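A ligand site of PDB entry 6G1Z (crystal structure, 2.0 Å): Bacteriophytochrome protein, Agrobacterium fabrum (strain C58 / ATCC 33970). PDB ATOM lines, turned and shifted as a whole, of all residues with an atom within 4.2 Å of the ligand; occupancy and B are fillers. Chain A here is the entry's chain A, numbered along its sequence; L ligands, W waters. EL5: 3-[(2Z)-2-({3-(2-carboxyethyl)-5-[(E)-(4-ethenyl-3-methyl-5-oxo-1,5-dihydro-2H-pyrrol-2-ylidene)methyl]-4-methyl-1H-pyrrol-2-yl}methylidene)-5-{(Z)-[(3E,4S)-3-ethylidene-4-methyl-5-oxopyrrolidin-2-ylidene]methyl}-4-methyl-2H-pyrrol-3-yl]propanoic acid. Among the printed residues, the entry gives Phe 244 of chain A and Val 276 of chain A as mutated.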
ATOM      1  N   LEU A  10      14.034 -23.555  32.405  1.00  0.00           N
ATOM      2  CA  LEU A  10      14.486 -22.572  33.402  1.00  0.00           C
ATOM      3  C   LEU A  10      15.360 -23.173  34.501  1.00  0.00           C
ATOM      4  O   LEU A  10      16.097 -22.428  35.161  1.00  0.00           O
ATOM      5  CB  LEU A  10      13.302 -21.840  34.016  1.00  0.00           C
ATOM      6  CG  LEU A  10      12.437 -21.046  33.041  1.00  0.00           C
ATOM      7  CD1 LEU A  10      11.391 -20.277  33.850  1.00  0.00           C
ATOM      8  CD2 LEU A  10      13.275 -20.109  32.172  1.00  0.00           C
ATOM      9  N   CYS A  13      19.006 -23.704  32.027  1.00  0.00           N
ATOM     10  CA  CYS A  13      19.439 -22.746  30.997  1.00  0.00           C
ATOM     11  C   CYS A  13      20.722 -22.008  31.361  1.00  0.00           C
ATOM     12  O   CYS A  13      21.468 -21.594  30.477  1.00  0.00           O
ATOM     13  CB  CYS A  13      18.321 -21.766  30.655  1.00  0.00           C
ATOM     14  SG  CYS A  13      17.729 -20.815  32.067  1.00  0.00           S
ATOM     15  N   ASP A  14      21.027 -21.897  32.663  1.00  0.00           N
ATOM     16  CA  ASP A  14      22.335 -21.365  33.093  1.00  0.00           C
ATOM     17  C   ASP A  14      23.531 -22.150  32.554  1.00  0.00           C
ATOM     18  O   ASP A  14      24.624 -21.614  32.472  1.00  0.00           O
ATOM     19  CB  ASP A  14      22.419 -21.287  34.633  1.00  0.00           C
ATOM     20  CG  ASP A  14      22.502 -22.672  35.289  1.00  0.00           C
ATOM     21  OD1 ASP A  14      21.721 -23.589  34.919  1.00  0.00           O
ATOM     22  OD2 ASP A  14      23.346 -22.839  36.199  1.00  0.00           O
ATOM     23  N   ILE A  18      25.443 -23.147  24.461  1.00  0.00           N
ATOM     24  CA  ILE A  18      24.964 -22.292  23.357  1.00  0.00           C
ATOM     25  C   ILE A  18      25.963 -22.096  22.232  1.00  0.00           C
ATOM     26  O   ILE A  18      25.597 -21.652  21.155  1.00  0.00           O
ATOM     27  CB  ILE A  18      24.483 -20.909  23.859  1.00  0.00           C
ATOM     28  CG1 ILE A  18      25.597 -20.179  24.634  1.00  0.00           C
ATOM     29  CG2 ILE A  18      23.221 -21.076  24.715  1.00  0.00           C
ATOM     30  CD1 ILE A  18      25.223 -18.767  25.042  1.00  0.00           C
ATOM     31  N   TYR A 165      23.787  -1.297  28.066  1.00  0.00           N
ATOM     32  CA  TYR A 165      23.825  -1.944  29.386  1.00  0.00           C
ATOM     33  C   TYR A 165      25.215  -1.841  29.953  1.00  0.00           C
ATOM     34  O   TYR A 165      26.183  -2.068  29.231  1.00  0.00           O
ATOM     35  CB  TYR A 165      23.539  -3.432  29.324  1.00  0.00           C
ATOM     36  CG  TYR A 165      22.353  -3.830  28.542  1.00  0.00           C
ATOM     37  CD1 TYR A 165      21.141  -3.173  28.687  1.00  0.00           C
ATOM     38  CD2 TYR A 165      22.415  -4.893  27.639  1.00  0.00           C
ATOM     39  CE1 TYR A 165      20.024  -3.548  27.941  1.00  0.00           C
ATOM     40  CE2 TYR A 165      21.309  -5.268  26.901  1.00  0.00           C
ATOM     41  CZ  TYR A 165      20.109  -4.591  27.052  1.00  0.00           C
ATOM     42  OH  TYR A 165      18.995  -4.964  26.326  1.00  0.00           O
ATOM     43  N   PHE A 187      13.030   1.392  29.097  1.00  0.00           N
ATOM     44  CA  PHE A 187      13.720   0.580  30.065  1.00  0.00           C
ATOM     45  C   PHE A 187      14.826   1.345  30.787  1.00  0.00           C
ATOM     46  O   PHE A 187      15.599   0.739  31.506  1.00  0.00           O
ATOM     47  CB  PHE A 187      14.324  -0.643  29.372  1.00  0.00           C
ATOM     48  CG  PHE A 187      13.293  -1.560  28.753  1.00  0.00           C
ATOM     49  CD1 PHE A 187      12.237  -2.051  29.518  1.00  0.00           C
ATOM     50  CD2 PHE A 187      13.391  -1.961  27.433  1.00  0.00           C
ATOM     51  CE1 PHE A 187      11.294  -2.902  28.978  1.00  0.00           C
ATOM     52  CE2 PHE A 187      12.455  -2.804  26.871  1.00  0.00           C
ATOM     53  CZ  PHE A 187      11.401  -3.274  27.644  1.00  0.00           C
ATOM     54  N   GLN A 190      16.507   0.792  34.488  1.00  0.00           N
ATOM     55  CA  GLN A 190      16.122  -0.547  34.911  1.00  0.00           C
ATOM     56  C   GLN A 190      17.359  -1.419  35.047  1.00  0.00           C
ATOM     57  O   GLN A 190      18.368  -1.166  34.404  1.00  0.00           O
ATOM     58  CB  GLN A 190      15.212  -1.139  33.840  1.00  0.00           C
ATOM     59  CG  GLN A 190      14.455  -2.341  34.258  1.00  0.00           C
ATOM     60  CD  GLN A 190      13.221  -2.584  33.409  1.00  0.00           C
ATOM     61  OE1 GLN A 190      12.473  -1.663  33.044  1.00  0.00           O
ATOM     62  NE2 GLN A 190      13.005  -3.849  33.078  1.00  0.00           N
ATOM     63  N   PHE A 192      18.662  -5.702  35.245  1.00  0.00           N
ATOM     64  CA  PHE A 192      18.347  -7.100  35.067  1.00  0.00           C
ATOM     65  C   PHE A 192      19.337  -7.985  35.854  1.00  0.00           C
ATOM     66  O   PHE A 192      20.492  -7.640  35.982  1.00  0.00           O
ATOM     67  CB  PHE A 192      18.243  -7.494  33.581  1.00  0.00           C
ATOM     68  CG  PHE A 192      19.498  -7.255  32.730  1.00  0.00           C
ATOM     69  CD1 PHE A 192      20.575  -8.133  32.774  1.00  0.00           C
ATOM     70  CD2 PHE A 192      19.543  -6.222  31.787  1.00  0.00           C
ATOM     71  CE1 PHE A 192      21.682  -7.949  31.956  1.00  0.00           C
ATOM     72  CE2 PHE A 192      20.648  -6.039  30.960  1.00  0.00           C
ATOM     73  CZ  PHE A 192      21.724  -6.902  31.053  1.00  0.00           C
ATOM     74  N   SER A 195      21.894 -13.478  36.012  1.00  0.00           N
ATOM     75  CA  SER A 195      21.491 -14.728  35.387  1.00  0.00           C
ATOM     76  C   SER A 195      20.736 -14.531  34.070  1.00  0.00           C
ATOM     77  O   SER A 195      20.623 -15.478  33.301  1.00  0.00           O
ATOM     78  CB  SER A 195      20.653 -15.565  36.349  1.00  0.00           C
ATOM     79  OG  SER A 195      19.431 -14.917  36.609  1.00  0.00           O
ATOM     80  N   ASP A 196      20.237 -13.325  33.785  1.00  0.00           N
ATOM     81  CA  ASP A 196      19.566 -13.099  32.479  1.00  0.00           C
ATOM     82  C   ASP A 196      20.496 -13.272  31.268  1.00  0.00           C
ATOM     83  O   ASP A 196      20.020 -13.482  30.162  1.00  0.00           O
ATOM     84  CB  ASP A 196      18.909 -11.708  32.411  1.00  0.00           C
ATOM     85  CG  ASP A 196      17.543 -11.649  33.101  1.00  0.00           C
ATOM     86  OD1 ASP A 196      17.255 -12.550  33.914  1.00  0.00           O
ATOM     87  OD2 ASP A 196      16.785 -10.677  32.835  1.00  0.00           O
ATOM     88  N   ILE A 197      21.803 -13.102  31.477  1.00  0.00           N
ATOM     89  CA  ILE A 197      22.799 -13.386  30.479  1.00  0.00           C
ATOM     90  C   ILE A 197      23.745 -14.416  31.113  1.00  0.00           C
ATOM     91  O   ILE A 197      24.563 -14.077  31.950  1.00  0.00           O
ATOM     92  CB  ILE A 197      23.572 -12.117  30.021  1.00  0.00           C
ATOM     93  CG1 ILE A 197      22.605 -11.023  29.537  1.00  0.00           C
ATOM     94  CG2 ILE A 197      24.522 -12.473  28.895  1.00  0.00           C
ATOM     95  CD1 ILE A 197      23.273  -9.733  29.168  1.00  0.00           C
ATOM     96  N   PRO A 198      23.610 -15.687  30.727  1.00  0.00           N
ATOM     97  CA  PRO A 198      24.451 -16.726  31.341  1.00  0.00           C
ATOM     98  C   PRO A 198      25.937 -16.594  30.988  1.00  0.00           C
ATOM     99  O   PRO A 198      26.300 -15.866  30.065  1.00  0.00           O
ATOM    100  CB  PRO A 198      23.889 -18.045  30.804  1.00  0.00           C
ATOM    101  CG  PRO A 198      22.853 -17.702  29.811  1.00  0.00           C
ATOM    102  CD  PRO A 198      22.514 -16.250  29.912  1.00  0.00           C
ATOM    103  N   ALA A 201      27.134 -17.070  27.528  1.00  0.00           N
ATOM    104  CA  ALA A 201      26.771 -15.941  26.673  1.00  0.00           C
ATOM    105  C   ALA A 201      27.774 -14.787  26.826  1.00  0.00           C
ATOM    106  O   ALA A 201      28.261 -14.258  25.836  1.00  0.00           O
ATOM    107  CB  ALA A 201      25.332 -15.478  26.951  1.00  0.00           C
ATOM    108  N   TYR A 205      30.125 -13.033  24.074  1.00  0.00           N
ATOM    109  CA  TYR A 205      30.134 -11.573  23.905  1.00  0.00           C
ATOM    110  C   TYR A 205      31.565 -11.024  24.003  1.00  0.00           C
ATOM    111  O   TYR A 205      31.942 -10.095  23.283  1.00  0.00           O
ATOM    112  CB  TYR A 205      29.224 -10.887  24.910  1.00  0.00           C
ATOM    113  CG  TYR A 205      27.745 -11.030  24.639  1.00  0.00           C
ATOM    114  CD1 TYR A 205      27.181 -10.659  23.392  1.00  0.00           C
ATOM    115  CD2 TYR A 205      26.879 -11.440  25.648  1.00  0.00           C
ATOM    116  CE1 TYR A 205      25.812 -10.760  23.158  1.00  0.00           C
ATOM    117  CE2 TYR A 205      25.520 -11.570  25.424  1.00  0.00           C
ATOM    118  CZ  TYR A 205      24.976 -11.230  24.176  1.00  0.00           C
ATOM    119  OH  TYR A 205      23.604 -11.326  23.983  1.00  0.00           O
ATOM    120  N   ARG A 211      27.118  -9.581  17.611  1.00  0.00           N
ATOM    121  CA  ARG A 211      26.215 -10.725  17.674  1.00  0.00           C
ATOM    122  C   ARG A 211      24.893 -10.327  16.996  1.00  0.00           C
ATOM    123  O   ARG A 211      24.308  -9.291  17.325  1.00  0.00           O
ATOM    124  CB  ARG A 211      26.055 -11.143  19.143  1.00  0.00           C
ATOM    125  CG  ARG A 211      24.957 -12.151  19.444  1.00  0.00           C
ATOM    126  CD  ARG A 211      25.062 -13.391  18.590  1.00  0.00           C
ATOM    127  NE  ARG A 211      24.180 -14.469  19.031  1.00  0.00           N
ATOM    128  CZ  ARG A 211      23.971 -15.589  18.327  1.00  0.00           C
ATOM    129  NH1 ARG A 211      24.546 -15.765  17.122  1.00  0.00           N
ATOM    130  NH2 ARG A 211      23.161 -16.524  18.802  1.00  0.00           N
ATOM    131  N   ILE A 213      21.001 -11.475  15.688  1.00  0.00           N
ATOM    132  CA  ILE A 213      19.803 -12.334  15.534  1.00  0.00           C
ATOM    133  C   ILE A 213      18.920 -11.703  14.435  1.00  0.00           C
ATOM    134  O   ILE A 213      18.333 -10.638  14.639  1.00  0.00           O
ATOM    135  CB  ILE A 213      19.034 -12.504  16.859  1.00  0.00           C
ATOM    136  CG1 ILE A 213      19.897 -13.245  17.870  1.00  0.00           C
ATOM    137  CG2 ILE A 213      17.743 -13.290  16.624  1.00  0.00           C
ATOM    138  CD1 ILE A 213      19.380 -13.198  19.302  1.00  0.00           C
ATOM    139  N   ARG A 242      25.593 -18.657  13.906  1.00  0.00           N
ATOM    140  CA  ARG A 242      25.215 -19.504  15.048  1.00  0.00           C
ATOM    141  C   ARG A 242      23.811 -19.163  15.535  1.00  0.00           C
ATOM    142  O   ARG A 242      23.498 -18.009  15.772  1.00  0.00           O
ATOM    143  CB  ARG A 242      26.196 -19.339  16.197  1.00  0.00           C
ATOM    144  CG  ARG A 242      25.854 -20.189  17.424  1.00  0.00           C
ATOM    145  CD  ARG A 242      26.937 -20.104  18.480  1.00  0.00           C
ATOM    146  NE  ARG A 242      27.209 -18.705  18.757  1.00  0.00           N
ATOM    147  CZ  ARG A 242      26.524 -17.950  19.592  1.00  0.00           C
ATOM    148  NH1 ARG A 242      26.881 -16.675  19.742  1.00  0.00           N
ATOM    149  NH2 ARG A 242      25.522 -18.456  20.318  1.00  0.00           N
ATOM    150  N   PHE A 244      20.524 -19.154  18.174  1.00  0.00           N
ATOM    151  CA  PHE A 244      20.439 -18.677  19.556  1.00  0.00           C
ATOM    152  C   PHE A 244      19.488 -19.568  20.359  1.00  0.00           C
ATOM    153  O   PHE A 244      18.629 -20.231  19.796  1.00  0.00           O
ATOM    154  CB  PHE A 244      19.948 -17.227  19.604  1.00  0.00           C
ATOM    155  CG  PHE A 244      18.653 -17.004  18.886  1.00  0.00           C
ATOM    156  CD1 PHE A 244      18.621 -16.948  17.487  1.00  0.00           C
ATOM    157  CD2 PHE A 244      17.459 -16.854  19.607  1.00  0.00           C
ATOM    158  CE1 PHE A 244      17.427 -16.762  16.825  1.00  0.00           C
ATOM    159  CE2 PHE A 244      16.274 -16.668  18.943  1.00  0.00           C
ATOM    160  CZ  PHE A 244      16.253 -16.631  17.554  1.00  0.00           C
ATOM    161  N   SER A 245      19.621 -19.503  21.677  1.00  0.00           N
ATOM    162  CA  SER A 245      18.808 -20.274  22.597  1.00  0.00           C
ATOM    163  C   SER A 245      17.313 -20.053  22.448  1.00  0.00           C
ATOM    164  O   SER A 245      16.844 -18.935  22.288  1.00  0.00           O
ATOM    165  CB  SER A 245      19.199 -19.929  24.044  1.00  0.00           C
ATOM    166  OG  SER A 245      18.193 -20.377  24.960  1.00  0.00           O
ATOM    167  N   ILE A 247      15.415 -20.134  24.917  1.00  0.00           N
ATOM    168  CA  ILE A 247      15.030 -19.370  26.103  1.00  0.00           C
ATOM    169  C   ILE A 247      15.006 -17.876  25.752  1.00  0.00           C
ATOM    170  O   ILE A 247      14.017 -17.183  25.996  1.00  0.00           O
ATOM    171  CB  ILE A 247      16.010 -19.604  27.269  1.00  0.00           C
ATOM    172  CG1 ILE A 247      16.053 -21.084  27.666  1.00  0.00           C
ATOM    173  CG2 ILE A 247      15.648 -18.720  28.450  1.00  0.00           C
ATOM    174  CD1 ILE A 247      14.735 -21.650  28.130  1.00  0.00           C
ATOM    175  N   HIS A 248      16.107 -17.388  25.173  1.00  0.00           N
ATOM    176  CA  HIS A 248      16.174 -16.020  24.674  1.00  0.00           C
ATOM    177  C   HIS A 248      15.164 -15.710  23.558  1.00  0.00           C
ATOM    178  O   HIS A 248      14.623 -14.611  23.505  1.00  0.00           O
ATOM    179  CB  HIS A 248      17.582 -15.708  24.197  1.00  0.00           C
ATOM    180  CG  HIS A 248      17.815 -14.261  23.925  1.00  0.00           C
ATOM    181  ND1 HIS A 248      17.599 -13.280  24.885  1.00  0.00           N
ATOM    182  CD2 HIS A 248      18.233 -13.612  22.815  1.00  0.00           C
ATOM    183  CE1 HIS A 248      17.889 -12.110  24.363  1.00  0.00           C
ATOM    184  NE2 HIS A 248      18.283 -12.278  23.110  1.00  0.00           N
ATOM    185  N   TYR A 251      12.017 -14.969  25.274  1.00  0.00           N
ATOM    186  CA  TYR A 251      12.153 -13.651  25.932  1.00  0.00           C
ATOM    187  C   TYR A 251      11.919 -12.542  24.901  1.00  0.00           C
ATOM    188  O   TYR A 251      11.104 -11.634  25.112  1.00  0.00           O
ATOM    189  CB  TYR A 251      13.539 -13.491  26.577  1.00  0.00           C
ATOM    190  CG  TYR A 251      13.573 -12.485  27.733  1.00  0.00           C
ATOM    191  CD1 TYR A 251      13.346 -11.136  27.516  1.00  0.00           C
ATOM    192  CD2 TYR A 251      13.860 -12.896  29.036  1.00  0.00           C
ATOM    193  CE1 TYR A 251      13.376 -10.241  28.561  1.00  0.00           C
ATOM    194  CE2 TYR A 251      13.894 -11.990  30.099  1.00  0.00           C
ATOM    195  CZ  TYR A 251      13.651 -10.663  29.856  1.00  0.00           C
ATOM    196  OH  TYR A 251      13.658  -9.740  30.882  1.00  0.00           O
ATOM    197  N   MET A 255       8.747  -9.716  24.384  1.00  0.00           N
ATOM    198  CA  MET A 255       8.982  -8.272  24.286  1.00  0.00           C
ATOM    199  C   MET A 255       8.448  -7.666  22.991  1.00  0.00           C
ATOM    200  O   MET A 255       8.409  -6.459  22.885  1.00  0.00           O
ATOM    201  CB  MET A 255      10.480  -7.944  24.403  1.00  0.00           C
ATOM    202  CG  MET A 255      11.080  -8.193  25.775  1.00  0.00           C
ATOM    203  SD  MET A 255      12.860  -7.946  25.724  1.00  0.00           S
ATOM    204  CE  MET A 255      12.821  -6.161  25.676  1.00  0.00           C
ATOM    205  N   LEU A 274      27.217  -3.770  26.877  1.00  0.00           N
ATOM    206  CA  LEU A 274      26.779  -4.018  25.491  1.00  0.00           C
ATOM    207  C   LEU A 274      26.023  -2.800  24.967  1.00  0.00           C
ATOM    208  O   LEU A 274      25.290  -2.152  25.728  1.00  0.00           O
ATOM    209  CB  LEU A 274      25.817  -5.196  25.404  1.00  0.00           C
ATOM    210  CG  LEU A 274      26.272  -6.546  25.966  1.00  0.00           C
ATOM    211  CD1 LEU A 274      25.088  -7.531  25.964  1.00  0.00           C
ATOM    212  CD2 LEU A 274      27.439  -7.124  25.178  1.00  0.00           C
ATOM    213  N   VAL A 276      23.068  -2.615  22.541  1.00  0.00           N
ATOM    214  CA  VAL A 276      22.101  -3.556  21.993  1.00  0.00           C
ATOM    215  C   VAL A 276      21.026  -2.855  21.169  1.00  0.00           C
ATOM    216  O   VAL A 276      20.361  -1.934  21.637  1.00  0.00           O
ATOM    217  CB  VAL A 276      21.456  -4.381  23.122  1.00  0.00           C
ATOM    218  CG1 VAL A 276      20.367  -5.300  22.575  1.00  0.00           C
ATOM    219  CG2 VAL A 276      22.526  -5.204  23.836  1.00  0.00           C
ATOM    220  N   HIS A 278      17.535  -3.433  19.171  1.00  0.00           N
ATOM    221  CA  HIS A 278      16.344  -4.279  19.055  1.00  0.00           C
ATOM    222  C   HIS A 278      15.443  -3.750  17.928  1.00  0.00           C
ATOM    223  O   HIS A 278      15.221  -2.541  17.825  1.00  0.00           O
ATOM    224  CB  HIS A 278      15.546  -4.261  20.347  1.00  0.00           C
ATOM    225  CG  HIS A 278      16.114  -5.119  21.435  1.00  0.00           C
ATOM    226  ND1 HIS A 278      15.617  -5.128  22.714  1.00  0.00           N
ATOM    227  CD2 HIS A 278      17.128  -6.022  21.421  1.00  0.00           C
ATOM    228  CE1 HIS A 278      16.302  -5.983  23.443  1.00  0.00           C
ATOM    229  NE2 HIS A 278      17.210  -6.554  22.682  1.00  0.00           N
ATOM    230  N   ARG A 456       8.800 -15.520  33.859  1.00  0.00           N
ATOM    231  CA  ARG A 456      10.229 -15.327  34.125  1.00  0.00           C
ATOM    232  C   ARG A 456      10.925 -14.597  32.965  1.00  0.00           C
ATOM    233  O   ARG A 456      11.849 -13.826  33.199  1.00  0.00           O
ATOM    234  CB  ARG A 456      10.939 -16.662  34.362  1.00  0.00           C
ATOM    235  CG  ARG A 456      12.463 -16.579  34.446  1.00  0.00           C
ATOM    236  CD  ARG A 456      12.914 -15.728  35.630  1.00  0.00           C
ATOM    237  NE  ARG A 456      14.372 -15.636  35.685  1.00  0.00           N
ATOM    238  CZ  ARG A 456      15.111 -14.666  35.149  1.00  0.00           C
ATOM    239  NH1 ARG A 456      14.539 -13.643  34.506  1.00  0.00           N
ATOM    240  NH2 ARG A 456      16.434 -14.696  35.271  1.00  0.00           N
ATOM    241  N   LEU A 457      10.475 -14.870  31.736  1.00  0.00           N
ATOM    242  CA  LEU A 457      11.097 -14.333  30.537  1.00  0.00           C
ATOM    243  C   LEU A 457      10.446 -13.030  30.077  1.00  0.00           C
ATOM    244  O   LEU A 457      10.053 -12.896  28.912  1.00  0.00           O
ATOM    245  CB  LEU A 457      11.041 -15.393  29.441  1.00  0.00           C
ATOM    246  CG  LEU A 457      11.657 -16.722  29.829  1.00  0.00           C
ATOM    247  CD1 LEU A 457      11.600 -17.699  28.654  1.00  0.00           C
ATOM    248  CD2 LEU A 457      13.083 -16.549  30.301  1.00  0.00           C
ATOM    249  N   PRO A 459      10.693  -8.488  30.953  1.00  0.00           N
ATOM    250  CA  PRO A 459      11.415  -7.439  31.639  1.00  0.00           C
ATOM    251  C   PRO A 459      10.843  -7.136  33.005  1.00  0.00           C
ATOM    252  O   PRO A 459      11.625  -6.868  33.937  1.00  0.00           O
ATOM    253  CB  PRO A 459      11.252  -6.241  30.699  1.00  0.00           C
ATOM    254  CG  PRO A 459      11.131  -6.844  29.327  1.00  0.00           C
ATOM    255  CD  PRO A 459      10.357  -8.115  29.561  1.00  0.00           C
ATOM    256  N   SER A 462      12.083  -9.861  35.379  1.00  0.00           N
ATOM    257  CA  SER A 462      13.541  -9.689  35.528  1.00  0.00           C
ATOM    258  C   SER A 462      13.861  -8.590  36.560  1.00  0.00           C
ATOM    259  O   SER A 462      14.625  -8.823  37.491  1.00  0.00           O
ATOM    260  CB  SER A 462      14.206  -9.370  34.168  1.00  0.00           C
ATOM    261  OG  SER A 462      14.366 -10.544  33.379  1.00  0.00           O
HETATM  262  C1A EL5 L   1      17.098 -15.359  30.610  1.00  0.00           C
HETATM  263  C1B EL5 L   1      20.132 -15.950  27.419  1.00  0.00           C
HETATM  264  O1B EL5 L   1      22.704 -16.175  21.603  1.00  0.00           O
HETATM  265  C1C EL5 L   1      20.059 -11.532  26.753  1.00  0.00           C
HETATM  266  O1C EL5 L   1      18.944  -8.597  23.253  1.00  0.00           O
HETATM  267  C1D EL5 L   1      17.069  -8.959  29.259  1.00  0.00           C
HETATM  268  C2A EL5 L   1      17.326 -16.561  31.518  1.00  0.00           C
HETATM  269  C2B EL5 L   1      21.019 -16.335  26.400  1.00  0.00           C
HETATM  270  O2B EL5 L   1      22.694 -13.953  21.305  1.00  0.00           O
HETATM  271  C2C EL5 L   1      20.423 -10.205  26.713  1.00  0.00           C
HETATM  272  O2C EL5 L   1      19.725  -7.430  25.061  1.00  0.00           O
HETATM  273  C2D EL5 L   1      16.574  -7.857  28.411  1.00  0.00           C
HETATM  274  C3A EL5 L   1      18.328 -17.222  30.677  1.00  0.00           C
HETATM  275  C3B EL5 L   1      21.339 -15.097  25.641  1.00  0.00           C
HETATM  276  C3C EL5 L   1      19.656  -9.621  27.630  1.00  0.00           C
HETATM  277  C3D EL5 L   1      15.807  -7.091  29.239  1.00  0.00           C
HETATM  278  C4A EL5 L   1      18.652 -16.439  29.582  1.00  0.00           C
HETATM  279  C4B EL5 L   1      20.719 -14.035  26.332  1.00  0.00           C
HETATM  280  C4C EL5 L   1      18.739 -10.632  28.142  1.00  0.00           C
HETATM  281  C4D EL5 L   1      15.856  -7.722  30.617  1.00  0.00           C
HETATM  282  CAA EL5 L   1      19.000 -18.461  30.963  1.00  0.00           C
HETATM  283  CAB EL5 L   1      22.162 -15.020  24.407  1.00  0.00           C
HETATM  284  CAC EL5 L   1      21.493  -9.520  25.876  1.00  0.00           C
HETATM  285  CAD EL5 L   1      15.178  -5.897  28.806  1.00  0.00           C
HETATM  286  CBA EL5 L   1      18.655 -19.274  32.167  1.00  0.00           C
HETATM  287  CBB EL5 L   1      21.340 -14.854  23.176  1.00  0.00           C
HETATM  288  CBC EL5 L   1      21.066  -9.364  24.306  1.00  0.00           C
HETATM  289  CBD EL5 L   1      14.655  -5.065  29.623  1.00  0.00           C
HETATM  290  CGB EL5 L   1      22.305 -15.001  21.926  1.00  0.00           C
HETATM  291  CGC EL5 L   1      19.827  -8.390  24.192  1.00  0.00           C
HETATM  292  CHB EL5 L   1      19.650 -16.767  28.547  1.00  0.00           C
HETATM  293  CHC EL5 L   1      20.624 -12.575  26.039  1.00  0.00           C
HETATM  294  CHD EL5 L   1      17.902 -10.178  29.258  1.00  0.00           C
HETATM  295  CMA EL5 L   1      16.114 -17.320  31.981  1.00  0.00           C
HETATM  296  CMB EL5 L   1      21.429 -17.661  26.059  1.00  0.00           C
HETATM  297  CMC EL5 L   1      19.713  -8.076  28.036  1.00  0.00           C
HETATM  298  CMD EL5 L   1      16.830  -7.612  26.940  1.00  0.00           C
HETATM  299  NA  EL5 L   1      17.899 -15.316  29.536  1.00  0.00           N
HETATM  300  OA  EL5 L   1      16.316 -14.470  30.837  1.00  0.00           O
HETATM  301  NB  EL5 L   1      19.992 -14.622  27.515  1.00  0.00           N
HETATM  302  NC  EL5 L   1      19.035 -11.814  27.707  1.00  0.00           N
HETATM  303  ND  EL5 L   1      16.552  -8.773  30.667  1.00  0.00           N
HETATM  304  OD  EL5 L   1      15.268  -7.271  31.646  1.00  0.00           O
HETATM  305  O   HOH W   1      21.274 -20.301  28.134  1.00  0.00           O
HETATM  306  O   HOH W   2      19.552 -10.308  21.461  1.00  0.00           O
HETATM  307  O   HOH W   3      21.928 -18.495  22.519  1.00  0.00           O
HETATM  308  O   HOH W   4      19.479 -19.240  35.248  1.00  0.00           O
HETATM  309  O   HOH W   5      21.497 -18.143  33.847  1.00  0.00           O
HETATM  310  O   HOH W   6      22.239 -11.190  21.631  1.00  0.00           O
HETATM  311  O   HOH W   7      16.846 -13.524  27.522  1.00  0.00           O
HETATM  312  O   HOH W   8      25.305 -16.122  22.071  1.00  0.00           O
HETATM  313  O   HOH W   9      14.883  -5.799  33.807  1.00  0.00           O
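Water W2 lies within hydrogen-bond range of O1C of the ligand and NE2 of His 248. Water W3 lies within hydrogen-bond range of an oxygen (O1B) of the ligand (2.6 Å) and the backbone NH (N) of Ser 245 (2.7 Å). Water W8 lies within hydrogen-bond range of an oxygen (O1B) of the ligand (2.6 Å) and the guanidinium group (NH1) of Arg 242 (2.9 Å). Water W9 lies within hydrogen-bond range of an oxygen (OD) of the ligand (2.6 Å), the side-chain amide nitrogen (NE2) of Gln 190 (2.8 Å) and the backbone carbonyl oxygen (O) of Pro 459 (3.4 Å). Water W7 bridges ND1 of His 248 (2.8 Å) and NC of the ligand (2.8 Å). Water W6 lies within hydrogen-bond range of OH of Tyr 205 and O2B of the ligand.
Merely in contact with the ligand: Pro 198, Tyr 205, Val 276, Ser 462, Leu 457, Phe 192, Phe 244, Asp 14, Ile 197, Pro 459, Ser 245, Ile 247, Phe 187, Ser 195, Met 255, Ile 213 and Leu 10. Hydrophobic or aromatic side chains that line the ligand: Leu 10, Tyr 165, Phe 187, Phe 192, Ile 197, Pro 198, Ile 213, Phe 244, Ile 247, His 248, Tyr 251, Met 255, Val 276, His 278, Leu 457 and Pro 459. Of the 30 residues printed, 25 come within 4 Å of the ligand. The nearest printed residue that does not touch the ligand is Gln 190 (4.02 Å).
The backbone carbonyl oxygen (O) of Arg 242 sits at hydrogen-bond distance from the guanidinium group (NH1) of Arg 211 (2.8 Å). The backbone carbonyl oxygen (O) of Leu 274 is in hydrogen-bond range of the backbone NH (N) of Tyr 165 (2.9 Å). The side-chain hydroxyl (OG) of Ser 195 sits at hydrogen-bond distance from the guanidinium group (NH2) of Arg 456 (3.3 Å). The side-chain hydroxyl (OH) of Tyr 251 is in hydrogen-bond range of the side-chain hydroxyl (OG) of Ser 462 (2.7 Å). NH2 of Arg 456 is in salt-bridge range of OD1 of Asp 196, 2.7 Å away. OG of Ser 245 sits at hydrogen-bond distance from N of Ile 247, at 2.8 Å. OD2 of Asp 196 sits at hydrogen-bond distance from OG of Ser 462 (2.5 Å). The backbone carbonyl oxygen (O) of Ile 18 is in hydrogen-bond range of the guanidinium group (NH2) of Arg 242 (3.3 Å).
OH of Tyr 165 sits at hydrogen-bond distance from O2C of the ligand (2.9 Å). An oxygen (OD) of the ligand lies close to the side-chain hydroxyl of Tyr 251 (3.0 Å). The guanidinium group of Arg 211 lies within salt-bridge range of an oxygen (O2B) of the ligand (2.8 Å). The side-chain sulfur of Cys 13 is bonded to a carbon (CBA) of the ligand, at 1.8 Å. A ring nitrogen (NE2) of His 278 lies within hydrogen-bond range of an oxygen (O1C) of the ligand (2.7 Å). ND of the ligand lies within hydrogen-bond range of OD2 of Asp 196 (2.9 Å). A ring nitrogen (ND1) of His 248 lies close to a nitrogen (NC) of the ligand (3.5 Å). The guanidinium group (NH2) of Arg 242 lies within salt-bridge range of an oxygen (O1B) of the ligand, 3.8 Å away. NA of the ligand is in hydrogen-bond range of O of Asp 196.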
